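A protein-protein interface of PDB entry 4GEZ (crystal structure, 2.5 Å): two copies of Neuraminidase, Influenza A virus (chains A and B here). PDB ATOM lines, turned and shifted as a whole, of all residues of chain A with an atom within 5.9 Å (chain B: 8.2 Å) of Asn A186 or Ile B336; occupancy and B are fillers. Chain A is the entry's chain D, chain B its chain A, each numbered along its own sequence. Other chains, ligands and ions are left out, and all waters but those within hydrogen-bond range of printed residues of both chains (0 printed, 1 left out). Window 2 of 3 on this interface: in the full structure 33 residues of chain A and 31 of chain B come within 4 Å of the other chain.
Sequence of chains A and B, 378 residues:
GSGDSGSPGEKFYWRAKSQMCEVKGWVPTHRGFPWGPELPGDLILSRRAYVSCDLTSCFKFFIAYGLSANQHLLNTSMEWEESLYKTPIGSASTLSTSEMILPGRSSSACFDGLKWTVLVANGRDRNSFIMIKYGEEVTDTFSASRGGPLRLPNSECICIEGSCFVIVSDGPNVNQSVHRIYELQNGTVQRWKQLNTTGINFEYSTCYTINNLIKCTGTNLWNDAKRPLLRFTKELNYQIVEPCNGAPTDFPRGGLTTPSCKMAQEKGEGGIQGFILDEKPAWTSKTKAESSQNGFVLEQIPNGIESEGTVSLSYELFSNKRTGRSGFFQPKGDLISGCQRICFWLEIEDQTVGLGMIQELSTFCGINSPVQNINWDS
No position is printed for both chains.
The side-chain carboxylate of Glu A137 lies within hydrogen-bond range of the backbone NH of Leu B335.
The backbone NH of Ile B336 lies within hydrogen-bond range of the side-chain carboxylate of Glu A137.
NH1 of Arg B341 is in salt-bridge range of OE1 of Glu A137 (3.9 Å).
Of the 14 printed residues of chain A, 4 touch a printed residue of chain B.
Among the printed residues, 7 pairs touch across the chains.
Among the printed residues, Asp or Glu carboxylates within 4 Å of a Lys or Arg side-chain nitrogen of the other chain: Glu A137 with Arg B341 (3.9 Å).
Asn A186 touches just one residue of chain B: Ile B336 (3.2 Å).
Ile B336 touches just these residues of chain A: Glu A137, Thr A139 and Asn A186.
No residue of chain B comes within 4 Å of Gly A187.
Printed residues of chain B within 4 Å of Glu A137: Asp B334, Leu B335, Ile B336 and Arg B341.
Printed residues of chain B within 4 Å of Val A138: Arg B341.
Of the printed residues of chain A, Asp B334 touches Glu A137 (3.1 Å).
Tyr A134 touches none of the printed residues of chain B.
Thr A188 touches none of the printed residues of chain B.
The nearest printed residue of chain A that does not touch Asp B334 is Val A138 (6.4 Å).
Among the printed residues, pairs that only touch across the chains: Glu A137 with Asp B334 (3.1 Å), Val A138 with Arg B341 (3.97 Å), Thr A139 with Ile B336 (3.7 Å) and Asn A186 with Ile B336 (3.2 Å).
The side-chain carboxylate (OD2) of Asp B334 is in salt-bridge range of the guanidinium group (NH1) of Arg B341 (2.7 Å).
The side-chain amide oxygen (OD1) of Asn A186 sits at hydrogen-bond distance from the side-chain hydroxyl (OH) of Tyr A13 (3.3 Å).
OG1 of Thr A139 lies within hydrogen-bond range of O of Gly A187 (2.5 Å).
The side-chain sulfur (SG) of Cys B339 forms a disulfide with the side-chain sulfur (SG) of Cys B21 (2.0 Å).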
ATOM      1  N   TYR A  13     -24.426 -33.852  22.931  1.00  0.00           N
ATOM      2  CA  TYR A  13     -23.119 -33.200  23.005  1.00  0.00           C
ATOM      3  C   TYR A  13     -22.037 -33.851  22.134  1.00  0.00           C
ATOM      4  O   TYR A  13     -21.305 -34.746  22.565  1.00  0.00           O
ATOM      5  CB  TYR A  13     -22.673 -33.022  24.461  1.00  0.00           C
ATOM      6  CG  TYR A  13     -23.294 -31.794  25.096  1.00  0.00           C
ATOM      7  CD1 TYR A  13     -23.986 -30.875  24.315  1.00  0.00           C
ATOM      8  CD2 TYR A  13     -23.170 -31.538  26.455  1.00  0.00           C
ATOM      9  CE1 TYR A  13     -24.549 -29.749  24.865  1.00  0.00           C
ATOM     10  CE2 TYR A  13     -23.732 -30.403  27.018  1.00  0.00           C
ATOM     11  CZ  TYR A  13     -24.422 -29.514  26.214  1.00  0.00           C
ATOM     12  OH  TYR A  13     -24.990 -28.382  26.752  1.00  0.00           O
ATOM     13  N   ASP A 112     -24.123 -27.993  18.359  1.00  0.00           N
ATOM     14  CA  ASP A 112     -23.445 -28.567  19.521  1.00  0.00           C
ATOM     15  C   ASP A 112     -23.782 -30.033  19.785  1.00  0.00           C
ATOM     16  O   ASP A 112     -23.133 -30.685  20.606  1.00  0.00           O
ATOM     17  CB  ASP A 112     -23.710 -27.729  20.780  1.00  0.00           C
ATOM     18  CG  ASP A 112     -25.175 -27.743  21.212  1.00  0.00           C
ATOM     19  OD1 ASP A 112     -26.011 -28.396  20.547  1.00  0.00           O
ATOM     20  OD2 ASP A 112     -25.488 -27.100  22.236  1.00  0.00           O
ATOM     21  N   THR A 117     -26.224 -22.907  17.482  1.00  0.00           N
ATOM     22  CA  THR A 117     -25.812 -21.610  17.995  1.00  0.00           C
ATOM     23  C   THR A 117     -25.559 -20.769  16.763  1.00  0.00           C
ATOM     24  O   THR A 117     -24.791 -21.160  15.885  1.00  0.00           O
ATOM     25  CB  THR A 117     -24.531 -21.691  18.849  1.00  0.00           C
ATOM     26  OG1 THR A 117     -24.783 -22.476  20.023  1.00  0.00           O
ATOM     27  CG2 THR A 117     -24.091 -20.302  19.284  1.00  0.00           C
ATOM     28  N   TYR A 134     -29.892 -19.326  20.265  1.00  0.00           N
ATOM     29  CA  TYR A 134     -29.713 -20.728  20.598  1.00  0.00           C
ATOM     30  C   TYR A 134     -31.059 -21.416  20.466  1.00  0.00           C
ATOM     31  O   TYR A 134     -31.904 -21.325  21.358  1.00  0.00           O
ATOM     32  CB  TYR A 134     -29.176 -20.872  22.021  1.00  0.00           C
ATOM     33  CG  TYR A 134     -28.740 -22.271  22.374  1.00  0.00           C
ATOM     34  CD1 TYR A 134     -27.567 -22.799  21.849  1.00  0.00           C
ATOM     35  CD2 TYR A 134     -29.489 -23.061  23.240  1.00  0.00           C
ATOM     36  CE1 TYR A 134     -27.153 -24.075  22.166  1.00  0.00           C
ATOM     37  CE2 TYR A 134     -29.082 -24.342  23.569  1.00  0.00           C
ATOM     38  CZ  TYR A 134     -27.912 -24.842  23.025  1.00  0.00           C
ATOM     39  OH  TYR A 134     -27.494 -26.114  23.339  1.00  0.00           O
ATOM     40  N   GLU A 137     -34.334 -18.934  20.040  1.00  0.00           N
ATOM     41  CA  GLU A 137     -34.344 -17.817  20.980  1.00  0.00           C
ATOM     42  C   GLU A 137     -33.004 -17.087  21.123  1.00  0.00           C
ATOM     43  O   GLU A 137     -31.937 -17.708  21.121  1.00  0.00           O
ATOM     44  CB  GLU A 137     -34.852 -18.303  22.345  1.00  0.00           C
ATOM     45  CG  GLU A 137     -33.933 -19.294  23.047  1.00  0.00           C
ATOM     46  CD  GLU A 137     -34.462 -19.704  24.405  1.00  0.00           C
ATOM     47  OE1 GLU A 137     -34.757 -18.800  25.216  1.00  0.00           O
ATOM     48  OE2 GLU A 137     -34.532 -20.923  24.678  1.00  0.00           O
ATOM     49  N   VAL A 138     -33.075 -15.764  21.269  1.00  0.00           N
ATOM     50  CA  VAL A 138     -31.882 -14.946  21.463  1.00  0.00           C
ATOM     51  C   VAL A 138     -31.459 -15.090  22.922  1.00  0.00           C
ATOM     52  O   VAL A 138     -32.265 -14.882  23.829  1.00  0.00           O
ATOM     53  CB  VAL A 138     -32.153 -13.463  21.132  1.00  0.00           C
ATOM     54  CG1 VAL A 138     -30.893 -12.637  21.322  1.00  0.00           C
ATOM     55  CG2 VAL A 138     -32.625 -13.323  19.706  1.00  0.00           C
ATOM     56  N   THR A 139     -30.198 -15.440  23.147  1.00  0.00           N
ATOM     57  CA  THR A 139     -29.741 -15.826  24.478  1.00  0.00           C
ATOM     58  C   THR A 139     -28.759 -14.825  25.067  1.00  0.00           C
ATOM     59  O   THR A 139     -28.696 -14.654  26.282  1.00  0.00           O
ATOM     60  CB  THR A 139     -29.079 -17.217  24.463  1.00  0.00           C
ATOM     61  OG1 THR A 139     -28.136 -17.288  23.385  1.00  0.00           O
ATOM     62  CG2 THR A 139     -30.125 -18.295  24.273  1.00  0.00           C
ATOM     63  N   GLY A 162     -20.146 -29.242  24.209  1.00  0.00           N
ATOM     64  CA  GLY A 162     -21.090 -28.241  24.663  1.00  0.00           C
ATOM     65  C   GLY A 162     -20.513 -26.843  24.714  1.00  0.00           C
ATOM     66  O   GLY A 162     -21.250 -25.880  24.912  1.00  0.00           O
ATOM     67  N   LEU A 184     -18.598 -20.021  24.251  1.00  0.00           N
ATOM     68  CA  LEU A 184     -20.019 -19.962  24.534  1.00  0.00           C
ATOM     69  C   LEU A 184     -20.524 -21.329  24.961  1.00  0.00           C
ATOM     70  O   LEU A 184     -19.987 -22.363  24.554  1.00  0.00           O
ATOM     71  CB  LEU A 184     -20.807 -19.486  23.305  1.00  0.00           C
ATOM     72  CG  LEU A 184     -20.310 -18.304  22.464  1.00  0.00           C
ATOM     73  CD1 LEU A 184     -21.200 -18.076  21.245  1.00  0.00           C
ATOM     74  CD2 LEU A 184     -20.226 -17.054  23.298  1.00  0.00           C
ATOM     75  N   GLN A 185     -21.564 -21.318  25.785  1.00  0.00           N
ATOM     76  CA  GLN A 185     -22.246 -22.531  26.194  1.00  0.00           C
ATOM     77  C   GLN A 185     -23.715 -22.183  26.339  1.00  0.00           C
ATOM     78  O   GLN A 185     -24.072 -21.236  27.050  1.00  0.00           O
ATOM     79  CB  GLN A 185     -21.676 -23.069  27.511  1.00  0.00           C
ATOM     80  CG  GLN A 185     -21.733 -24.593  27.608  1.00  0.00           C
ATOM     81  CD  GLN A 185     -20.983 -25.160  28.803  1.00  0.00           C
ATOM     82  OE1 GLN A 185     -19.929 -24.657  29.190  1.00  0.00           O
ATOM     83  NE2 GLN A 185     -21.517 -26.233  29.378  1.00  0.00           N
ATOM     84  N   ASN A 186     -24.558 -22.958  25.661  1.00  0.00           N
ATOM     85  CA  ASN A 186     -25.996 -22.712  25.605  1.00  0.00           C
ATOM     86  C   ASN A 186     -26.333 -21.306  25.102  1.00  0.00           C
ATOM     87  O   ASN A 186     -27.259 -20.659  25.588  1.00  0.00           O
ATOM     88  CB  ASN A 186     -26.633 -22.977  26.972  1.00  0.00           C
ATOM     89  CG  ASN A 186     -26.410 -24.401  27.452  1.00  0.00           C
ATOM     90  OD1 ASN A 186     -26.309 -25.333  26.652  1.00  0.00           O
ATOM     91  ND2 ASN A 186     -26.313 -24.574  28.765  1.00  0.00           N
ATOM     92  N   GLY A 187     -25.549 -20.837  24.134  1.00  0.00           N
ATOM     93  CA  GLY A 187     -25.762 -19.536  23.525  1.00  0.00           C
ATOM     94  C   GLY A 187     -25.417 -18.363  24.425  1.00  0.00           C
ATOM     95  O   GLY A 187     -25.804 -17.224  24.155  1.00  0.00           O
ATOM     96  N   THR A 188     -24.670 -18.637  25.489  1.00  0.00           N
ATOM     97  CA  THR A 188     -24.288 -17.606  26.448  1.00  0.00           C
ATOM     98  C   THR A 188     -22.767 -17.519  26.563  1.00  0.00           C
ATOM     99  O   THR A 188     -22.089 -18.548  26.645  1.00  0.00           O
ATOM    100  CB  THR A 188     -24.902 -17.883  27.842  1.00  0.00           C
ATOM    101  OG1 THR A 188     -26.334 -17.866  27.753  1.00  0.00           O
ATOM    102  CG2 THR A 188     -24.457 -16.834  28.844  1.00  0.00           C
ATOM    103  N   GLN A 190     -19.348 -17.489  28.030  1.00  0.00           N
ATOM    104  CA  GLN A 190     -18.746 -17.975  29.263  1.00  0.00           C
ATOM    105  C   GLN A 190     -17.540 -17.121  29.589  1.00  0.00           C
ATOM    106  O   GLN A 190     -17.383 -16.648  30.714  1.00  0.00           O
ATOM    107  CB  GLN A 190     -18.347 -19.443  29.136  1.00  0.00           C
ATOM    108  CG  GLN A 190     -19.525 -20.343  28.858  1.00  0.00           C
ATOM    109  CD  GLN A 190     -20.629 -20.141  29.873  1.00  0.00           C
ATOM    110  OE1 GLN A 190     -20.438 -20.378  31.066  1.00  0.00           O
ATOM    111  NE2 GLN A 190     -21.787 -19.682  29.409  1.00  0.00           N
ATOM    112  N   CYS B  21     -39.085 -11.722  32.560  1.00  0.00           N
ATOM    113  CA  CYS B  21     -37.663 -11.429  32.475  1.00  0.00           C
ATOM    114  C   CYS B  21     -37.502  -9.921  32.549  1.00  0.00           C
ATOM    115  O   CYS B  21     -38.361  -9.180  32.069  1.00  0.00           O
ATOM    116  CB  CYS B  21     -37.067 -11.955  31.165  1.00  0.00           C
ATOM    117  SG  CYS B  21     -37.078 -13.753  30.987  1.00  0.00           S
ATOM    118  N   GLY B 333     -41.819 -21.803  24.725  1.00  0.00           N
ATOM    119  CA  GLY B 333     -40.747 -22.778  24.648  1.00  0.00           C
ATOM    120  C   GLY B 333     -39.611 -22.284  25.522  1.00  0.00           C
ATOM    121  O   GLY B 333     -39.649 -22.467  26.737  1.00  0.00           O
ATOM    122  N   ASP B 334     -38.616 -21.651  24.900  1.00  0.00           N
ATOM    123  CA  ASP B 334     -37.502 -20.998  25.602  1.00  0.00           C
ATOM    124  C   ASP B 334     -36.912 -21.786  26.780  1.00  0.00           C
ATOM    125  O   ASP B 334     -37.322 -21.607  27.928  1.00  0.00           O
ATOM    126  CB  ASP B 334     -37.916 -19.592  26.056  1.00  0.00           C
ATOM    127  CG  ASP B 334     -38.258 -18.678  24.892  1.00  0.00           C
ATOM    128  OD1 ASP B 334     -37.932 -19.036  23.739  1.00  0.00           O
ATOM    129  OD2 ASP B 334     -38.841 -17.598  25.130  1.00  0.00           O
ATOM    130  N   LEU B 335     -35.941 -22.645  26.485  1.00  0.00           N
ATOM    131  CA  LEU B 335     -35.326 -23.502  27.500  1.00  0.00           C
ATOM    132  C   LEU B 335     -34.051 -22.950  28.154  1.00  0.00           C
ATOM    133  O   LEU B 335     -33.341 -23.694  28.832  1.00  0.00           O
ATOM    134  CB  LEU B 335     -35.058 -24.903  26.928  1.00  0.00           C
ATOM    135  CG  LEU B 335     -36.231 -25.899  26.883  1.00  0.00           C
ATOM    136  CD1 LEU B 335     -37.393 -25.423  26.017  1.00  0.00           C
ATOM    137  CD2 LEU B 335     -35.757 -27.278  26.431  1.00  0.00           C
ATOM    138  N   ILE B 336     -33.761 -21.663  27.973  1.00  0.00           N
ATOM    139  CA  ILE B 336     -32.550 -21.084  28.563  1.00  0.00           C
ATOM    140  C   ILE B 336     -32.899 -20.155  29.722  1.00  0.00           C
ATOM    141  O   ILE B 336     -32.131 -20.018  30.674  1.00  0.00           O
ATOM    142  CB  ILE B 336     -31.673 -20.325  27.530  1.00  0.00           C
ATOM    143  CG1 ILE B 336     -30.342 -19.911  28.157  1.00  0.00           C
ATOM    144  CG2 ILE B 336     -32.366 -19.071  27.049  1.00  0.00           C
ATOM    145  CD1 ILE B 336     -29.270 -20.947  28.045  1.00  0.00           C
ATOM    146  N   SER B 337     -34.076 -19.545  29.654  1.00  0.00           N
ATOM    147  CA  SER B 337     -34.523 -18.665  30.720  1.00  0.00           C
ATOM    148  C   SER B 337     -35.599 -19.348  31.552  1.00  0.00           C
ATOM    149  O   SER B 337     -36.471 -20.034  31.018  1.00  0.00           O
ATOM    150  CB  SER B 337     -35.043 -17.337  30.159  1.00  0.00           C
ATOM    151  OG  SER B 337     -36.063 -17.544  29.198  1.00  0.00           O
ATOM    152  N   GLY B 338     -35.529 -19.162  32.864  1.00  0.00           N
ATOM    153  CA  GLY B 338     -36.539 -19.699  33.755  1.00  0.00           C
ATOM    154  C   GLY B 338     -37.597 -18.632  33.941  1.00  0.00           C
ATOM    155  O   GLY B 338     -38.560 -18.810  34.688  1.00  0.00           O
ATOM    156  N   CYS B 339     -37.408 -17.520  33.238  1.00  0.00           N
ATOM    157  CA  CYS B 339     -38.350 -16.412  33.259  1.00  0.00           C
ATOM    158  C   CYS B 339     -39.072 -16.296  31.919  1.00  0.00           C
ATOM    159  O   CYS B 339     -38.583 -16.771  30.893  1.00  0.00           O
ATOM    160  CB  CYS B 339     -37.623 -15.104  33.603  1.00  0.00           C
ATOM    161  SG  CYS B 339     -36.203 -14.722  32.544  1.00  0.00           S
ATOM    162  N   ARG B 341     -40.184 -14.719  28.627  1.00  0.00           N
ATOM    163  CA  ARG B 341     -39.795 -13.691  27.674  1.00  0.00           C
ATOM    164  C   ARG B 341     -41.022 -13.022  27.063  1.00  0.00           C
ATOM    165  O   ARG B 341     -42.101 -13.617  26.981  1.00  0.00           O
ATOM    166  CB  ARG B 341     -38.889 -14.264  26.572  1.00  0.00           C
ATOM    167  CG  ARG B 341     -37.404 -14.249  26.933  1.00  0.00           C
ATOM    168  CD  ARG B 341     -36.526 -15.034  25.953  1.00  0.00           C
ATOM    169  NE  ARG B 341     -36.419 -14.402  24.637  1.00  0.00           N
ATOM    170  CZ  ARG B 341     -36.752 -14.989  23.489  1.00  0.00           C
ATOM    171  NH1 ARG B 341     -37.205 -16.233  23.483  1.00  0.00           N
ATOM    172  NH2 ARG B 341     -36.621 -14.336  22.342  1.00  0.00           N
